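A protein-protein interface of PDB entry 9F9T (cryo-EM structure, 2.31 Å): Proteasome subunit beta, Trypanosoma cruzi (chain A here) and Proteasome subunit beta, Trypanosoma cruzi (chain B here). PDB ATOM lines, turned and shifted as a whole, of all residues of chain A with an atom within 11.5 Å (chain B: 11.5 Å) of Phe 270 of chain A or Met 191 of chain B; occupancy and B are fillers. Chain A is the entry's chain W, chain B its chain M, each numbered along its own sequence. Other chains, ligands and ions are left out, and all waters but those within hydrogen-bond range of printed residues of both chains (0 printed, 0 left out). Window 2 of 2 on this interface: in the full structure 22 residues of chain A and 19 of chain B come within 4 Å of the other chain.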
ATOM      1  N   GLN A 266      10.187  11.465  21.923  1.00  0.00           N
ATOM      2  CA  GLN A 266      11.537  10.971  21.703  1.00  0.00           C
ATOM      3  C   GLN A 266      11.408   9.692  20.885  1.00  0.00           C
ATOM      4  O   GLN A 266      10.623   8.805  21.213  1.00  0.00           O
ATOM      5  CB  GLN A 266      12.297  10.719  23.012  1.00  0.00           C
ATOM      6  CG  GLN A 266      13.778  10.364  22.832  1.00  0.00           C
ATOM      7  CD  GLN A 266      14.458   9.882  24.099  1.00  0.00           C
ATOM      8  OE1 GLN A 266      14.845   8.720  24.213  1.00  0.00           O
ATOM      9  NE2 GLN A 266      14.620  10.770  25.071  1.00  0.00           N
ATOM     10  N   GLU A 267      12.167   9.629  19.795  1.00  0.00           N
ATOM     11  CA  GLU A 267      12.191   8.443  18.967  1.00  0.00           C
ATOM     12  C   GLU A 267      13.237   7.514  19.576  1.00  0.00           C
ATOM     13  O   GLU A 267      14.386   7.899  19.771  1.00  0.00           O
ATOM     14  CB  GLU A 267      12.432   8.849  17.507  1.00  0.00           C
ATOM     15  CG  GLU A 267      11.393   8.291  16.539  1.00  0.00           C
ATOM     16  CD  GLU A 267      11.298   8.993  15.189  1.00  0.00           C
ATOM     17  OE1 GLU A 267      10.161   9.363  14.787  1.00  0.00           O
ATOM     18  OE2 GLU A 267      12.352   9.160  14.538  1.00  0.00           O
ATOM     19  N   ILE A 268      12.796   6.307  19.925  1.00  0.00           N
ATOM     20  CA  ILE A 268      13.657   5.254  20.440  1.00  0.00           C
ATOM     21  C   ILE A 268      13.782   4.207  19.348  1.00  0.00           C
ATOM     22  O   ILE A 268      12.757   3.785  18.827  1.00  0.00           O
ATOM     23  CB  ILE A 268      13.063   4.645  21.726  1.00  0.00           C
ATOM     24  CG1 ILE A 268      12.737   5.731  22.756  1.00  0.00           C
ATOM     25  CG2 ILE A 268      13.975   3.564  22.285  1.00  0.00           C
ATOM     26  CD1 ILE A 268      11.947   5.255  23.942  1.00  0.00           C
ATOM     27  N   ARG A 269      15.027   3.828  19.023  1.00  0.00           N
ATOM     28  CA  ARG A 269      15.328   2.977  17.880  1.00  0.00           C
ATOM     29  C   ARG A 269      15.894   1.649  18.359  1.00  0.00           C
ATOM     30  O   ARG A 269      16.711   1.612  19.273  1.00  0.00           O
ATOM     31  CB  ARG A 269      16.400   3.574  16.956  1.00  0.00           C
ATOM     32  CG  ARG A 269      16.123   4.985  16.457  1.00  0.00           C
ATOM     33  CD  ARG A 269      14.722   5.130  15.894  1.00  0.00           C
ATOM     34  NE  ARG A 269      14.550   6.326  15.072  1.00  0.00           N
ATOM     35  CZ  ARG A 269      14.993   6.468  13.822  1.00  0.00           C
ATOM     36  NH1 ARG A 269      15.752   5.534  13.272  1.00  0.00           N
ATOM     37  NH2 ARG A 269      14.670   7.549  13.130  1.00  0.00           N
ATOM     38  N   PHE A 270      15.465   0.573  17.695  1.00  0.00           N
ATOM     39  CA  PHE A 270      16.153  -0.697  17.778  1.00  0.00           C
ATOM     40  C   PHE A 270      16.685  -1.027  16.386  1.00  0.00           C
ATOM     41  O   PHE A 270      15.892  -1.273  15.480  1.00  0.00           O
ATOM     42  CB  PHE A 270      15.240  -1.773  18.384  1.00  0.00           C
ATOM     43  CG  PHE A 270      14.836  -1.506  19.816  1.00  0.00           C
ATOM     44  CD1 PHE A 270      15.775  -1.084  20.760  1.00  0.00           C
ATOM     45  CD2 PHE A 270      13.516  -1.660  20.225  1.00  0.00           C
ATOM     46  CE1 PHE A 270      15.404  -0.789  22.065  1.00  0.00           C
ATOM     47  CE2 PHE A 270      13.156  -1.390  21.542  1.00  0.00           C
ATOM     48  CZ  PHE A 270      14.099  -0.963  22.460  1.00  0.00           C
ATOM     49  N   PRO A 271      18.033  -1.021  16.187  1.00  0.00           N
ATOM     50  CA  PRO A 271      18.645  -1.606  14.990  1.00  0.00           C
ATOM     51  C   PRO A 271      18.246  -3.073  14.794  1.00  0.00           C
ATOM     52  O   PRO A 271      18.525  -3.898  15.659  1.00  0.00           O
ATOM     53  CB  PRO A 271      20.169  -1.524  15.234  1.00  0.00           C
ATOM     54  CG  PRO A 271      20.350  -1.096  16.695  1.00  0.00           C
ATOM     55  CD  PRO A 271      19.032  -0.489  17.127  1.00  0.00           C
ATOM     56  N   PRO A 272      17.596  -3.457  13.668  1.00  0.00           N
ATOM     57  CA  PRO A 272      17.293  -4.862  13.360  1.00  0.00           C
ATOM     58  C   PRO A 272      18.388  -5.897  13.648  1.00  0.00           C
ATOM     59  O   PRO A 272      19.505  -5.765  13.149  1.00  0.00           O
ATOM     60  CB  PRO A 272      17.043  -4.803  11.842  1.00  0.00           C
ATOM     61  CG  PRO A 272      16.419  -3.448  11.622  1.00  0.00           C
ATOM     62  CD  PRO A 272      17.112  -2.543  12.620  1.00  0.00           C
ATOM     63  N   GLY A 273      18.047  -6.942  14.431  1.00  0.00           N
ATOM     64  CA  GLY A 273      19.029  -7.833  15.048  1.00  0.00           C
ATOM     65  C   GLY A 273      19.343  -7.495  16.517  1.00  0.00           C
ATOM     66  O   GLY A 273      20.358  -7.933  17.050  1.00  0.00           O
ATOM     67  N   THR A 274      18.428  -6.775  17.176  1.00  0.00           N
ATOM     68  CA  THR A 274      18.507  -6.373  18.578  1.00  0.00           C
ATOM     69  C   THR A 274      17.994  -7.528  19.461  1.00  0.00           C
ATOM     70  O   THR A 274      18.574  -7.827  20.519  1.00  0.00           O
ATOM     71  CB  THR A 274      17.802  -5.010  18.741  1.00  0.00           C
ATOM     72  OG1 THR A 274      18.707  -3.936  18.477  1.00  0.00           O
ATOM     73  CG2 THR A 274      17.237  -4.757  20.119  1.00  0.00           C
ATOM     74  N   THR A 275      16.959  -8.236  18.967  1.00  0.00           N
ATOM     75  CA  THR A 275      16.297  -9.340  19.653  1.00  0.00           C
ATOM     76  C   THR A 275      16.890 -10.684  19.185  1.00  0.00           C
ATOM     77  O   THR A 275      16.940 -10.965  17.999  1.00  0.00           O
ATOM     78  CB  THR A 275      14.771  -9.179  19.495  1.00  0.00           C
ATOM     79  OG1 THR A 275      14.411  -7.863  19.940  1.00  0.00           O
ATOM     80  CG2 THR A 275      13.960 -10.198  20.276  1.00  0.00           C
ATOM     81  N   PRO A 276      17.441 -11.536  20.092  1.00  0.00           N
ATOM     82  CA  PRO A 276      17.859 -12.904  19.763  1.00  0.00           C
ATOM     83  C   PRO A 276      16.771 -13.910  19.358  1.00  0.00           C
ATOM     84  O   PRO A 276      15.934 -14.313  20.157  1.00  0.00           O
ATOM     85  CB  PRO A 276      18.495 -13.411  21.074  1.00  0.00           C
ATOM     86  CG  PRO A 276      18.953 -12.152  21.760  1.00  0.00           C
ATOM     87  CD  PRO A 276      17.818 -11.201  21.476  1.00  0.00           C
ATOM     88  N   VAL A 277      16.851 -14.362  18.113  1.00  0.00           N
ATOM     89  CA  VAL A 277      15.914 -15.334  17.579  1.00  0.00           C
ATOM     90  C   VAL A 277      16.568 -16.722  17.623  1.00  0.00           C
ATOM     91  O   VAL A 277      17.741 -16.908  17.283  1.00  0.00           O
ATOM     92  CB  VAL A 277      15.485 -14.846  16.182  1.00  0.00           C
ATOM     93  CG1 VAL A 277      14.822 -15.909  15.343  1.00  0.00           C
ATOM     94  CG2 VAL A 277      14.603 -13.613  16.300  1.00  0.00           C
ATOM     95  N   GLU B 179       7.210   0.628  34.474  1.00  0.00           N
ATOM     96  CA  GLU B 179       8.306  -0.147  35.058  1.00  0.00           C
ATOM     97  C   GLU B 179       8.950  -1.104  34.074  1.00  0.00           C
ATOM     98  O   GLU B 179      10.152  -1.107  33.925  1.00  0.00           O
ATOM     99  CB  GLU B 179       7.871  -0.881  36.313  1.00  0.00           C
ATOM    100  CG  GLU B 179       8.949  -0.928  37.357  1.00  0.00           C
ATOM    101  CD  GLU B 179       8.602  -1.581  38.698  1.00  0.00           C
ATOM    102  OE1 GLU B 179       7.549  -2.247  38.797  1.00  0.00           O
ATOM    103  OE2 GLU B 179       9.411  -1.397  39.669  1.00  0.00           O
ATOM    104  N   PRO B 180       8.219  -1.882  33.242  1.00  0.00           N
ATOM    105  CA  PRO B 180       8.868  -2.649  32.180  1.00  0.00           C
ATOM    106  C   PRO B 180       9.615  -1.783  31.187  1.00  0.00           C
ATOM    107  O   PRO B 180      10.484  -2.287  30.491  1.00  0.00           O
ATOM    108  CB  PRO B 180       7.779  -3.391  31.411  1.00  0.00           C
ATOM    109  CG  PRO B 180       6.523  -3.122  32.176  1.00  0.00           C
ATOM    110  CD  PRO B 180       6.781  -2.158  33.316  1.00  0.00           C
ATOM    111  N   LEU B 181       9.237  -0.509  31.064  1.00  0.00           N
ATOM    112  CA  LEU B 181       9.881   0.311  30.065  1.00  0.00           C
ATOM    113  C   LEU B 181      11.238   0.675  30.617  1.00  0.00           C
ATOM    114  O   LEU B 181      12.231   0.587  29.907  1.00  0.00           O
ATOM    115  CB  LEU B 181       9.004   1.502  29.693  1.00  0.00           C
ATOM    116  CG  LEU B 181       9.654   2.613  28.856  1.00  0.00           C
ATOM    117  CD1 LEU B 181       9.870   2.099  27.431  1.00  0.00           C
ATOM    118  CD2 LEU B 181       8.775   3.908  28.845  1.00  0.00           C
ATOM    119  N   MET B 182      11.312   0.906  31.913  1.00  0.00           N
ATOM    120  CA  MET B 182      12.588   1.273  32.484  1.00  0.00           C
ATOM    121  C   MET B 182      13.452   0.018  32.584  1.00  0.00           C
ATOM    122  O   MET B 182      14.652   0.079  32.438  1.00  0.00           O
ATOM    123  CB  MET B 182      12.375   1.798  33.906  1.00  0.00           C
ATOM    124  CG  MET B 182      11.856   3.231  34.014  1.00  0.00           C
ATOM    125  SD  MET B 182      11.421   3.422  35.803  1.00  0.00           S
ATOM    126  CE  MET B 182      11.612   5.183  36.008  1.00  0.00           C
ATOM    127  N   ASP B 183      12.837  -1.129  32.878  1.00  0.00           N
ATOM    128  CA  ASP B 183      13.578  -2.368  32.868  1.00  0.00           C
ATOM    129  C   ASP B 183      14.253  -2.475  31.506  1.00  0.00           C
ATOM    130  O   ASP B 183      15.468  -2.508  31.432  1.00  0.00           O
ATOM    131  CB  ASP B 183      12.727  -3.607  33.173  1.00  0.00           C
ATOM    132  CG  ASP B 183      12.174  -3.864  34.590  1.00  0.00           C
ATOM    133  OD1 ASP B 183      12.847  -3.548  35.591  1.00  0.00           O
ATOM    134  OD2 ASP B 183      11.086  -4.532  34.659  1.00  0.00           O
ATOM    135  N   CYS B 184      13.472  -2.433  30.436  1.00  0.00           N
ATOM    136  CA  CYS B 184      13.972  -2.432  29.061  1.00  0.00           C
ATOM    137  C   CYS B 184      15.116  -1.428  28.834  1.00  0.00           C
ATOM    138  O   CYS B 184      16.190  -1.820  28.391  1.00  0.00           O
ATOM    139  CB  CYS B 184      12.821  -2.224  28.060  1.00  0.00           C
ATOM    140  SG  CYS B 184      13.229  -2.513  26.309  1.00  0.00           S
ATOM    141  N   LEU B 185      14.921  -0.150  29.029  1.00  0.00           N
ATOM    142  CA  LEU B 185      15.889   0.817  28.487  1.00  0.00           C
ATOM    143  C   LEU B 185      17.166   0.858  29.330  1.00  0.00           C
ATOM    144  O   LEU B 185      18.231   1.093  28.784  1.00  0.00           O
ATOM    145  CB  LEU B 185      15.259   2.217  28.420  1.00  0.00           C
ATOM    146  CG  LEU B 185      13.946   2.313  27.626  1.00  0.00           C
ATOM    147  CD1 LEU B 185      13.354   3.734  27.654  1.00  0.00           C
ATOM    148  CD2 LEU B 185      14.147   1.834  26.176  1.00  0.00           C
ATOM    149  N   LEU B 186      17.073   0.614  30.650  1.00  0.00           N
ATOM    150  CA  LEU B 186      18.228   0.668  31.549  1.00  0.00           C
ATOM    151  C   LEU B 186      18.942  -0.666  31.684  1.00  0.00           C
ATOM    152  O   LEU B 186      20.158  -0.653  31.781  1.00  0.00           O
ATOM    153  CB  LEU B 186      17.784   1.107  32.933  1.00  0.00           C
ATOM    154  CG  LEU B 186      17.118   2.463  32.944  1.00  0.00           C
ATOM    155  CD1 LEU B 186      16.386   2.675  34.255  1.00  0.00           C
ATOM    156  CD2 LEU B 186      18.162   3.550  32.652  1.00  0.00           C
ATOM    157  N   THR B 187      18.269  -1.814  31.665  1.00  0.00           N
ATOM    158  CA  THR B 187      19.038  -3.040  31.888  1.00  0.00           C
ATOM    159  C   THR B 187      19.356  -3.781  30.589  1.00  0.00           C
ATOM    160  O   THR B 187      20.339  -4.519  30.576  1.00  0.00           O
ATOM    161  CB  THR B 187      18.429  -3.918  33.005  1.00  0.00           C
ATOM    162  OG1 THR B 187      17.122  -4.400  32.707  1.00  0.00           O
ATOM    163  CG2 THR B 187      18.312  -3.152  34.309  1.00  0.00           C
ATOM    164  N   ARG B 188      18.467  -3.683  29.582  1.00  0.00           N
ATOM    165  CA  ARG B 188      18.629  -4.226  28.225  1.00  0.00           C
ATOM    166  C   ARG B 188      18.920  -5.736  28.222  1.00  0.00           C
ATOM    167  O   ARG B 188      19.921  -6.180  27.674  1.00  0.00           O
ATOM    168  CB  ARG B 188      19.748  -3.460  27.507  1.00  0.00           C
ATOM    169  CG  ARG B 188      19.769  -1.957  27.779  1.00  0.00           C
ATOM    170  CD  ARG B 188      20.871  -1.209  27.065  1.00  0.00           C
ATOM    171  NE  ARG B 188      20.581  -1.028  25.657  1.00  0.00           N
ATOM    172  CZ  ARG B 188      21.373  -0.383  24.810  1.00  0.00           C
ATOM    173  NH1 ARG B 188      20.982  -0.188  23.563  1.00  0.00           N
ATOM    174  NH2 ARG B 188      22.546   0.080  25.218  1.00  0.00           N
ATOM    175  N   GLN B 189      18.067  -6.530  28.876  1.00  0.00           N
ATOM    176  CA  GLN B 189      18.402  -7.915  29.139  1.00  0.00           C
ATOM    177  C   GLN B 189      18.114  -8.744  27.883  1.00  0.00           C
ATOM    178  O   GLN B 189      18.790  -9.736  27.649  1.00  0.00           O
ATOM    179  CB  GLN B 189      17.731  -8.429  30.425  1.00  0.00           C
ATOM    180  CG  GLN B 189      16.665  -9.504  30.210  1.00  0.00           C
ATOM    181  CD  GLN B 189      16.389 -10.406  31.403  1.00  0.00           C
ATOM    182  OE1 GLN B 189      16.669 -11.610  31.380  1.00  0.00           O
ATOM    183  NE2 GLN B 189      15.779  -9.832  32.435  1.00  0.00           N
ATOM    184  N   HIS B 190      17.188  -8.291  27.027  1.00  0.00           N
ATOM    185  CA  HIS B 190      16.829  -9.025  25.816  1.00  0.00           C
ATOM    186  C   HIS B 190      17.410  -8.358  24.567  1.00  0.00           C
ATOM    187  O   HIS B 190      16.752  -8.385  23.519  1.00  0.00           O
ATOM    188  CB  HIS B 190      15.304  -9.218  25.688  1.00  0.00           C
ATOM    189  CG  HIS B 190      14.688  -9.855  26.887  1.00  0.00           C
ATOM    190  ND1 HIS B 190      15.048 -11.112  27.336  1.00  0.00           N
ATOM    191  CD2 HIS B 190      13.783  -9.393  27.759  1.00  0.00           C
ATOM    192  CE1 HIS B 190      14.365 -11.401  28.434  1.00  0.00           C
ATOM    193  NE2 HIS B 190      13.597 -10.378  28.711  1.00  0.00           N
ATOM    194  N   MET B 191      18.650  -7.828  24.688  1.00  0.00           N
ATOM    195  CA  MET B 191      19.375  -7.199  23.582  1.00  0.00           C
ATOM    196  C   MET B 191      20.776  -7.783  23.476  1.00  0.00           C
ATOM    197  O   MET B 191      21.164  -8.582  24.327  1.00  0.00           O
ATOM    198  CB  MET B 191      19.451  -5.689  23.774  1.00  0.00           C
ATOM    199  CG  MET B 191      18.066  -5.080  23.755  1.00  0.00           C
ATOM    200  SD  MET B 191      18.039  -3.294  23.879  1.00  0.00           S
ATOM    201  CE  MET B 191      16.448  -3.030  24.668  1.00  0.00           C
ATOM    202  N   VAL B 192      21.513  -7.380  22.423  1.00  0.00           N
ATOM    203  CA  VAL B 192      22.846  -7.900  22.128  1.00  0.00           C
ATOM    204  C   VAL B 192      23.929  -6.846  22.470  1.00  0.00           C
ATOM    205  O   VAL B 192      23.625  -5.610  22.517  1.00  0.00           O
ATOM    206  CB  VAL B 192      22.910  -8.389  20.659  1.00  0.00           C
ATOM    207  CG1 VAL B 192      24.102  -9.296  20.411  1.00  0.00           C
ATOM    208  CG2 VAL B 192      21.634  -9.105  20.217  1.00  0.00           C
ATOM    209  N   MET B 207      14.561  10.489  29.481  1.00  0.00           N
ATOM    210  CA  MET B 207      13.904   9.192  29.582  1.00  0.00           C
ATOM    211  C   MET B 207      12.709   9.273  30.527  1.00  0.00           C
ATOM    212  O   MET B 207      11.644   8.753  30.273  1.00  0.00           O
ATOM    213  CB  MET B 207      14.882   8.147  30.116  1.00  0.00           C
ATOM    214  CG  MET B 207      14.228   6.799  30.514  1.00  0.00           C
ATOM    215  SD  MET B 207      15.493   5.586  30.980  1.00  0.00           S
ATOM    216  CE  MET B 207      16.727   5.800  29.688  1.00  0.00           C
ATOM    217  N   ASN B 210       9.912  11.177  28.998  1.00  0.00           N
ATOM    218  CA  ASN B 210       9.220  10.412  27.999  1.00  0.00           C
ATOM    219  C   ASN B 210       8.279   9.408  28.647  1.00  0.00           C
ATOM    220  O   ASN B 210       7.224   9.123  28.107  1.00  0.00           O
ATOM    221  CB  ASN B 210      10.212   9.752  27.056  1.00  0.00           C
ATOM    222  CG  ASN B 210       9.470   9.414  25.783  1.00  0.00           C
ATOM    223  OD1 ASN B 210       8.865  10.310  25.170  1.00  0.00           O
ATOM    224  ND2 ASN B 210       9.453   8.124  25.426  1.00  0.00           N
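No residue of chain B comes within 4 Å of Ile 268 of chain A. Arg 269 of chain A touches none of the printed residues of chain B. Phe 270 of chain A touches one residue of chain B. No residue of chain B comes within 4 Å of Pro 271 of chain A. No residue of chain B comes within 4 Å of Pro 272 of chain A. Of chain B, only Val 192 (3.6 Å) comes within 4 Å of Gly 273 of chain A. Thr 274 of chain A touches just these residues of chain B: His 190, Met 191 and Val 192. Printed residues of chain B within 4 Å of Pro 276 of chain A: His 190. No residue of chain A comes within 4 Å of Cys 184 of chain B. Gln 189 of chain B touches none of the printed residues of chain A. Of the printed residues of chain A, His 190 of chain B touches Thr 274 and Pro 276. Met 191 of chain B touches just these residues of chain A: Phe 270 and Thr 274. The nearest printed residue of chain A that does not touch Asn 210 of chain B is Ile 268 of chain A (4.1 Å).
O of Pro 271 of chain A lies within hydrogen-bond range of OG1 of Thr 274 of chain A (2.8 Å).
Hydrophobic or aromatic side chains of chain A within 4 Å of the printed part of chain B: Phe 270 and Pro 276. Along chain A the printed residues that touch a printed residue of chain B span positions 266 to 276. Hydrophobic or aromatic side chains of chain B within 4 Å of the printed part of chain A: Met 191 and Val 192. Among the printed residues, no Asp or Glu carboxylate lies within 4 Å of a Lys or Arg side-chain nitrogen of the other chain.
Gln 266 of chain A touches Asn 210 of chain B (N to OD1, 3.7 Å). CE1 of Phe 270 of chain A touches CE of Met 191 of chain B (3.6 Å). Gly 273 of chain A touches Val 192 of chain B. Thr 274 of chain A touches His 190 of chain B. Thr 274 of chain A touches Met 191 of chain B (O to CA, 3.2 Å). O of Thr 274 of chain A touches CG2 of Val 192 of chain B, 3.3 Å away. CD of Pro 276 of chain A touches O of His 190 of chain B, 3.6 Å away.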
